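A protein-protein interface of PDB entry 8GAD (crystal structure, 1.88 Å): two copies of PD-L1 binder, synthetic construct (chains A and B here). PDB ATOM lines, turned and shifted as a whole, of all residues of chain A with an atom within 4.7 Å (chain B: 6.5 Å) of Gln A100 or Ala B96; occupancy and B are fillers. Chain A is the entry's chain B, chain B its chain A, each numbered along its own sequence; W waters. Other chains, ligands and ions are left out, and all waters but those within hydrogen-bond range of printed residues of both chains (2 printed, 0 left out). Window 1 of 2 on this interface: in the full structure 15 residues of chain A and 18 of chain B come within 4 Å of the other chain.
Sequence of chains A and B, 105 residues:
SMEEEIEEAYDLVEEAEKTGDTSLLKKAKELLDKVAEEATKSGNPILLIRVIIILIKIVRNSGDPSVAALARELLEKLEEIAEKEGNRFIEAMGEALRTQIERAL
Of chain B, only Ala B96 and Thr B99 come within 4 Å of Gln A100.
Ala B96 touches just one residue of chain A: Gln A100 (3.8 Å).
Of the printed residues of chain A, Gln B100 touches Ala A96 (3.6 Å).
Of the printed residues of chain B, Arg A103 touches Thr B99 (3.4 Å).
Ile B101 touches none of the printed residues of chain A.
Thr A99 touches none of the printed residues of chain B.
The nearest residue of chain A that does not touch Ala B96 is Ala A96 (4.1 Å).
The nearest printed residue of chain B that does not touch Arg A103 is Glu B95 (5.3 Å).
Ala A96 touches Gln B100, and with the chains exchanged Gln A100 touches Ala B96.
Gln A100 touches Thr B99, but with the chains exchanged Thr A99 does not touch Gln B100 (5.1 Å).
Positions printed for both chains: 56, 96, 97, 98, 99, 100 and 101.
O of Glu B95 lies within hydrogen-bond range of OG1 of Thr B99 (3.1 Å).
The side-chain amide oxygen (OE1) of Gln A100 is in hydrogen-bond range of the guanidinium group (NH2) of Arg A60 (3.0 Å).
OE1 of Gln A100 is in hydrogen-bond range of NH2 of Arg A103 (3.2 Å).
Among the printed residues, pairs that only touch across the chains: Ala A96 with Gln B100 (3.6 Å) and Gln A100 with Ala B96 (3.8 Å).
Hydrophobic or aromatic side chains of chain A within 4 Å of the printed part of chain B: Ala A96.
Among the printed residues, 4 pairs touch across the chains.
Among the printed residues, no Asp or Glu carboxylate lies within 4 Å of a Lys or Arg side-chain nitrogen of the other chain.
Water W1 lies within hydrogen-bond range of the backbone carbonyl oxygen (O) of Ala A96 (2.8 Å), the backbone carbonyl oxygen (O) of Ala B96 (2.8 Å) and the side-chain amide nitrogen (NE2) of Gln A100 (3.0 Å).
Water W2 lies within hydrogen-bond range of the backbone carbonyl oxygen (O) of Ala B92 and the side-chain amide oxygen (OE1) of Gln A100.
NE2 of Gln A100 sits at hydrogen-bond distance from OG1 of Thr B99 (3.3 Å).
The guanidinium group (NH2) of Arg A103 sits at hydrogen-bond distance from the side-chain hydroxyl (OG1) of Thr B99.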
ATOM      1  N   ILE A  56     -18.374  -8.078   4.155  1.00  0.00           N
ATOM      2  CA  ILE A  56     -19.385  -8.738   3.323  1.00  0.00           C
ATOM      3  C   ILE A  56     -18.743  -9.810   2.444  1.00  0.00           C
ATOM      4  O   ILE A  56     -19.285 -10.910   2.289  1.00  0.00           O
ATOM      5  CB  ILE A  56     -20.141  -7.700   2.477  1.00  0.00           C
ATOM      6  CG1 ILE A  56     -20.994  -6.812   3.388  1.00  0.00           C
ATOM      7  CG2 ILE A  56     -21.013  -8.402   1.431  1.00  0.00           C
ATOM      8  CD1 ILE A  56     -21.577  -5.586   2.696  1.00  0.00           C
ATOM      9  N   ARG A  60     -19.717 -13.786   2.402  1.00  0.00           N
ATOM     10  CA  ARG A  60     -20.024 -14.577   1.209  1.00  0.00           C
ATOM     11  C   ARG A  60     -19.189 -15.848   1.153  1.00  0.00           C
ATOM     12  O   ARG A  60     -19.693 -16.917   0.788  1.00  0.00           O
ATOM     13  CB  ARG A  60     -19.784 -13.759  -0.059  1.00  0.00           C
ATOM     14  CG  ARG A  60     -20.847 -12.747  -0.359  1.00  0.00           C
ATOM     15  CD  ARG A  60     -20.591 -12.064  -1.682  1.00  0.00           C
ATOM     16  NE  ARG A  60     -21.476 -10.918  -1.842  1.00  0.00           N
ATOM     17  CZ  ARG A  60     -21.060  -9.709  -2.189  1.00  0.00           C
ATOM     18  NH1 ARG A  60     -19.776  -9.457  -2.406  1.00  0.00           N
ATOM     19  NH2 ARG A  60     -21.945  -8.718  -2.275  1.00  0.00           N
ATOM     20  N   ALA A  96     -28.094   0.143   1.441  1.00  0.00           N
ATOM     21  CA  ALA A  96     -27.788  -0.738   0.316  1.00  0.00           C
ATOM     22  C   ALA A  96     -26.809  -1.828   0.728  1.00  0.00           C
ATOM     23  O   ALA A  96     -26.901  -2.961   0.248  1.00  0.00           O
ATOM     24  CB  ALA A  96     -27.227   0.065  -0.865  1.00  0.00           C
ATOM     25  N   LEU A  97     -25.851  -1.494   1.603  1.00  0.00           N
ATOM     26  CA  LEU A  97     -24.918  -2.511   2.098  1.00  0.00           C
ATOM     27  C   LEU A  97     -25.585  -3.454   3.082  1.00  0.00           C
ATOM     28  O   LEU A  97     -25.240  -4.642   3.131  1.00  0.00           O
ATOM     29  CB  LEU A  97     -23.699  -1.861   2.755  1.00  0.00           C
ATOM     30  CG  LEU A  97     -22.800  -1.056   1.804  1.00  0.00           C
ATOM     31  CD1 LEU A  97     -21.768  -0.282   2.604  1.00  0.00           C
ATOM     32  CD2 LEU A  97     -22.120  -1.973   0.812  1.00  0.00           C
ATOM     33  N   ARG A  98     -26.518  -2.951   3.899  1.00  0.00           N
ATOM     34  CA  ARG A  98     -27.263  -3.842   4.787  1.00  0.00           C
ATOM     35  C   ARG A  98     -27.893  -4.980   3.994  1.00  0.00           C
ATOM     36  O   ARG A  98     -27.820  -6.150   4.395  1.00  0.00           O
ATOM     37  CB  ARG A  98     -28.335  -3.058   5.551  1.00  0.00           C
ATOM     38  CG  ARG A  98     -29.045  -3.887   6.607  1.00  0.00           C
ATOM     39  CD  ARG A  98     -30.188  -3.109   7.273  1.00  0.00           C
ATOM     40  NE  ARG A  98     -29.696  -1.915   7.951  1.00  0.00           N
ATOM     41  CZ  ARG A  98     -29.116  -1.907   9.145  1.00  0.00           C
ATOM     42  NH1 ARG A  98     -28.933  -3.025   9.833  1.00  0.00           N
ATOM     43  NH2 ARG A  98     -28.704  -0.748   9.660  1.00  0.00           N
ATOM     44  N   THR A  99     -28.489  -4.651   2.843  1.00  0.00           N
ATOM     45  CA  THR A  99     -29.038  -5.678   1.958  1.00  0.00           C
ATOM     46  C   THR A  99     -27.968  -6.681   1.543  1.00  0.00           C
ATOM     47  O   THR A  99     -28.232  -7.887   1.472  1.00  0.00           O
ATOM     48  CB  THR A  99     -29.652  -5.015   0.724  1.00  0.00           C
ATOM     49  OG1 THR A  99     -30.740  -4.176   1.127  1.00  0.00           O
ATOM     50  CG2 THR A  99     -30.155  -6.061  -0.271  1.00  0.00           C
ATOM     51  N   GLN A 100     -26.750  -6.202   1.263  1.00  0.00           N
ATOM     52  CA  GLN A 100     -25.718  -7.108   0.768  1.00  0.00           C
ATOM     53  C   GLN A 100     -25.303  -8.101   1.849  1.00  0.00           C
ATOM     54  O   GLN A 100     -25.025  -9.266   1.549  1.00  0.00           O
ATOM     55  CB  GLN A 100     -24.499  -6.333   0.259  1.00  0.00           C
ATOM     56  CG  GLN A 100     -24.752  -5.459  -0.977  1.00  0.00           C
ATOM     57  CD  GLN A 100     -25.097  -6.248  -2.246  1.00  0.00           C
ATOM     58  OE1 GLN A 100     -24.256  -6.949  -2.817  1.00  0.00           O
ATOM     59  NE2 GLN A 100     -26.344  -6.113  -2.702  1.00  0.00           N
ATOM     60  N   ILE A 101     -25.248  -7.657   3.112  1.00  0.00           N
ATOM     61  CA  ILE A 101     -24.923  -8.573   4.210  1.00  0.00           C
ATOM     62  C   ILE A 101     -25.931  -9.703   4.270  1.00  0.00           C
ATOM     63  O   ILE A 101     -25.569 -10.883   4.349  1.00  0.00           O
ATOM     64  CB  ILE A 101     -24.868  -7.833   5.558  1.00  0.00           C
ATOM     65  CG1 ILE A 101     -23.676  -6.898   5.627  1.00  0.00           C
ATOM     66  CG2 ILE A 101     -24.796  -8.818   6.709  1.00  0.00           C
ATOM     67  CD1 ILE A 101     -23.793  -5.968   6.798  1.00  0.00           C
ATOM     68  N   GLU A 102     -27.217  -9.352   4.266  1.00  0.00           N
ATOM     69  CA  GLU A 102     -28.248 -10.367   4.455  1.00  0.00           C
ATOM     70  C   GLU A 102     -28.236 -11.369   3.311  1.00  0.00           C
ATOM     71  O   GLU A 102     -28.334 -12.581   3.532  1.00  0.00           O
ATOM     72  CB  GLU A 102     -29.617  -9.698   4.579  1.00  0.00           C
ATOM     73  CG  GLU A 102     -29.751  -8.737   5.777  1.00  0.00           C
ATOM     74  CD  GLU A 102     -29.210  -9.307   7.095  1.00  0.00           C
ATOM     75  OE1 GLU A 102     -29.216 -10.546   7.284  1.00  0.00           O
ATOM     76  OE2 GLU A 102     -28.761  -8.499   7.941  1.00  0.00           O
ATOM     77  N   ARG A 103     -28.087 -10.878   2.081  1.00  0.00           N
ATOM     78  CA  ARG A 103     -28.052 -11.752   0.917  1.00  0.00           C
ATOM     79  C   ARG A 103     -26.785 -12.613   0.878  1.00  0.00           C
ATOM     80  O   ARG A 103     -26.774 -13.657   0.210  1.00  0.00           O
ATOM     81  CB  ARG A 103     -28.231 -10.879  -0.337  1.00  0.00           C
ATOM     82  CG  ARG A 103     -27.871 -11.512  -1.668  1.00  0.00           C
ATOM     83  CD  ARG A 103     -28.175 -10.564  -2.820  1.00  0.00           C
ATOM     84  NE  ARG A 103     -26.937 -10.058  -3.398  1.00  0.00           N
ATOM     85  CZ  ARG A 103     -26.820  -9.530  -4.607  1.00  0.00           C
ATOM     86  NH1 ARG A 103     -27.804  -9.600  -5.490  1.00  0.00           N
ATOM     87  NH2 ARG A 103     -25.683  -8.922  -4.939  1.00  0.00           N
ATOM     88  N   ALA A 104     -25.735 -12.232   1.615  1.00  0.00           N
ATOM     89  CA  ALA A 104     -24.499 -13.006   1.644  1.00  0.00           C
ATOM     90  C   ALA A 104     -24.546 -14.164   2.633  1.00  0.00           C
ATOM     91  O   ALA A 104     -23.730 -15.091   2.537  1.00  0.00           O
ATOM     92  CB  ALA A 104     -23.323 -12.094   1.989  1.00  0.00           C
ATOM     93  N   ILE B  56     -32.705   6.003  -7.866  1.00  0.00           N
ATOM     94  CA  ILE B  56     -33.320   4.824  -7.266  1.00  0.00           C
ATOM     95  C   ILE B  56     -34.565   5.221  -6.480  1.00  0.00           C
ATOM     96  O   ILE B  56     -35.618   4.583  -6.587  1.00  0.00           O
ATOM     97  CB  ILE B  56     -32.308   4.085  -6.372  1.00  0.00           C
ATOM     98  CG1 ILE B  56     -31.285   3.353  -7.242  1.00  0.00           C
ATOM     99  CG2 ILE B  56     -33.030   3.099  -5.440  1.00  0.00           C
ATOM    100  CD1 ILE B  56     -30.093   2.804  -6.497  1.00  0.00           C
ATOM    101  N   GLU B  91     -16.343  -0.289  -7.005  1.00  0.00           N
ATOM    102  CA  GLU B  91     -16.992  -1.408  -7.685  1.00  0.00           C
ATOM    103  C   GLU B  91     -18.069  -2.032  -6.800  1.00  0.00           C
ATOM    104  O   GLU B  91     -19.193  -2.288  -7.253  1.00  0.00           O
ATOM    105  CB  GLU B  91     -15.948  -2.457  -8.090  1.00  0.00           C
ATOM    106  CG  GLU B  91     -16.538  -3.641  -8.834  1.00  0.00           C
ATOM    107  CD  GLU B  91     -15.498  -4.701  -9.203  1.00  0.00           C
ATOM    108  OE1 GLU B  91     -14.548  -4.932  -8.416  1.00  0.00           O
ATOM    109  OE2 GLU B  91     -15.623  -5.293 -10.297  1.00  0.00           O
ATOM    110  N   ALA B  92     -17.745  -2.270  -5.526  1.00  0.00           N
ATOM    111  CA  ALA B  92     -18.714  -2.885  -4.625  1.00  0.00           C
ATOM    112  C   ALA B  92     -19.898  -1.961  -4.367  1.00  0.00           C
ATOM    113  O   ALA B  92     -21.040  -2.428  -4.272  1.00  0.00           O
ATOM    114  CB  ALA B  92     -18.046  -3.264  -3.302  1.00  0.00           C
ATOM    115  N   MET B  93     -19.654  -0.655  -4.209  1.00  0.00           N
ATOM    116  CA  MET B  93     -20.783   0.259  -4.026  1.00  0.00           C
ATOM    117  C   MET B  93     -21.675   0.282  -5.256  1.00  0.00           C
ATOM    118  O   MET B  93     -22.908   0.316  -5.137  1.00  0.00           O
ATOM    119  CB  MET B  93     -20.310   1.675  -3.661  1.00  0.00           C
ATOM    120  CG  MET B  93     -19.761   1.743  -2.241  1.00  0.00           C
ATOM    121  SD  MET B  93     -19.342   3.422  -1.719  1.00  0.00           S
ATOM    122  CE  MET B  93     -18.062   3.804  -2.908  1.00  0.00           C
ATOM    123  N   GLY B  94     -21.076   0.253  -6.443  1.00  0.00           N
ATOM    124  CA  GLY B  94     -21.877   0.162  -7.650  1.00  0.00           C
ATOM    125  C   GLY B  94     -22.721  -1.097  -7.684  1.00  0.00           C
ATOM    126  O   GLY B  94     -23.886  -1.057  -8.078  1.00  0.00           O
ATOM    127  N   GLU B  95     -22.148  -2.234  -7.280  1.00  0.00           N
ATOM    128  CA  GLU B  95     -22.920  -3.482  -7.291  1.00  0.00           C
ATOM    129  C   GLU B  95     -24.073  -3.417  -6.299  1.00  0.00           C
ATOM    130  O   GLU B  95     -25.158  -3.950  -6.558  1.00  0.00           O
ATOM    131  CB  GLU B  95     -21.998  -4.671  -6.980  1.00  0.00           C
ATOM    132  CG  GLU B  95     -21.330  -5.296  -8.207  1.00  0.00           C
ATOM    133  CD  GLU B  95     -22.198  -5.214  -9.473  1.00  0.00           C
ATOM    134  OE1 GLU B  95     -23.255  -5.886  -9.514  1.00  0.00           O
ATOM    135  OE2 GLU B  95     -21.845  -4.461 -10.413  1.00  0.00           O
ATOM    136  N   ALA B  96     -23.848  -2.786  -5.145  1.00  0.00           N
ATOM    137  CA  ALA B  96     -24.907  -2.686  -4.150  1.00  0.00           C
ATOM    138  C   ALA B  96     -26.047  -1.820  -4.663  1.00  0.00           C
ATOM    139  O   ALA B  96     -27.222  -2.127  -4.421  1.00  0.00           O
ATOM    140  CB  ALA B  96     -24.356  -2.130  -2.832  1.00  0.00           C
ATOM    141  N   LEU B  97     -25.723  -0.745  -5.393  1.00  0.00           N
ATOM    142  CA  LEU B  97     -26.769   0.104  -5.957  1.00  0.00           C
ATOM    143  C   LEU B  97     -27.475  -0.603  -7.104  1.00  0.00           C
ATOM    144  O   LEU B  97     -28.685  -0.429  -7.305  1.00  0.00           O
ATOM    145  CB  LEU B  97     -26.180   1.435  -6.431  1.00  0.00           C
ATOM    146  CG  LEU B  97     -25.638   2.338  -5.321  1.00  0.00           C
ATOM    147  CD1 LEU B  97     -25.024   3.560  -5.960  1.00  0.00           C
ATOM    148  CD2 LEU B  97     -26.719   2.747  -4.328  1.00  0.00           C
ATOM    149  N   ARG B  98     -26.743  -1.413  -7.866  1.00  0.00           N
ATOM    150  CA  ARG B  98     -27.381  -2.104  -8.978  1.00  0.00           C
ATOM    151  C   ARG B  98     -28.390  -3.136  -8.482  1.00  0.00           C
ATOM    152  O   ARG B  98     -29.431  -3.343  -9.114  1.00  0.00           O
ATOM    153  CB  ARG B  98     -26.324  -2.752  -9.876  1.00  0.00           C
ATOM    154  CG  ARG B  98     -26.928  -3.643 -10.958  1.00  0.00           C
ATOM    155  CD  ARG B  98     -25.868  -4.512 -11.643  1.00  0.00           C
ATOM    156  NE  ARG B  98     -24.833  -3.740 -12.327  1.00  0.00           N
ATOM    157  CZ  ARG B  98     -25.028  -2.748 -13.192  1.00  0.00           C
ATOM    158  NH1 ARG B  98     -26.241  -2.392 -13.587  1.00  0.00           N
ATOM    159  NH2 ARG B  98     -23.971  -2.115 -13.703  1.00  0.00           N
ATOM    160  N   THR B  99     -28.105  -3.798  -7.357  1.00  0.00           N
ATOM    161  CA  THR B  99     -29.095  -4.694  -6.763  1.00  0.00           C
ATOM    162  C   THR B  99     -30.403  -3.963  -6.474  1.00  0.00           C
ATOM    163  O   THR B  99     -31.495  -4.513  -6.679  1.00  0.00           O
ATOM    164  CB  THR B  99     -28.536  -5.300  -5.477  1.00  0.00           C
ATOM    165  OG1 THR B  99     -27.361  -6.055  -5.795  1.00  0.00           O
ATOM    166  CG2 THR B  99     -29.563  -6.235  -4.839  1.00  0.00           C
ATOM    167  N   GLN B 100     -30.310  -2.725  -5.995  1.00  0.00           N
ATOM    168  CA  GLN B 100     -31.505  -1.944  -5.691  1.00  0.00           C
ATOM    169  C   GLN B 100     -32.295  -1.618  -6.954  1.00  0.00           C
ATOM    170  O   GLN B 100     -33.524  -1.760  -6.980  1.00  0.00           O
ATOM    171  CB  GLN B 100     -31.105  -0.669  -4.958  1.00  0.00           C
ATOM    172  CG  GLN B 100     -30.452  -0.932  -3.607  1.00  0.00           C
ATOM    173  CD  GLN B 100     -30.373   0.322  -2.775  1.00  0.00           C
ATOM    174  OE1 GLN B 100     -29.988   1.384  -3.277  1.00  0.00           O
ATOM    175  NE2 GLN B 100     -30.745   0.221  -1.502  1.00  0.00           N
ATOM    176  N   ILE B 101     -31.610  -1.157  -8.007  1.00  0.00           N
ATOM    177  CA  ILE B 101     -32.279  -0.926  -9.294  1.00  0.00           C
ATOM    178  C   ILE B 101     -32.983  -2.184  -9.773  1.00  0.00           C
ATOM    179  O   ILE B 101     -34.131  -2.139 -10.227  1.00  0.00           O
ATOM    180  CB  ILE B 101     -31.274  -0.428 -10.354  1.00  0.00           C
ATOM    181  CG1 ILE B 101     -30.782   0.968 -10.022  1.00  0.00           C
ATOM    182  CG2 ILE B 101     -31.921  -0.404 -11.729  1.00  0.00           C
ATOM    183  CD1 ILE B 101     -31.948   1.954 -10.108  1.00  0.00           C
HETATM  184  O   HOH W   1     -27.980  -3.687  -2.218  1.00  0.00           O
HETATM  185  O   HOH W   2     -21.706  -4.935  -3.095  1.00  0.00           O
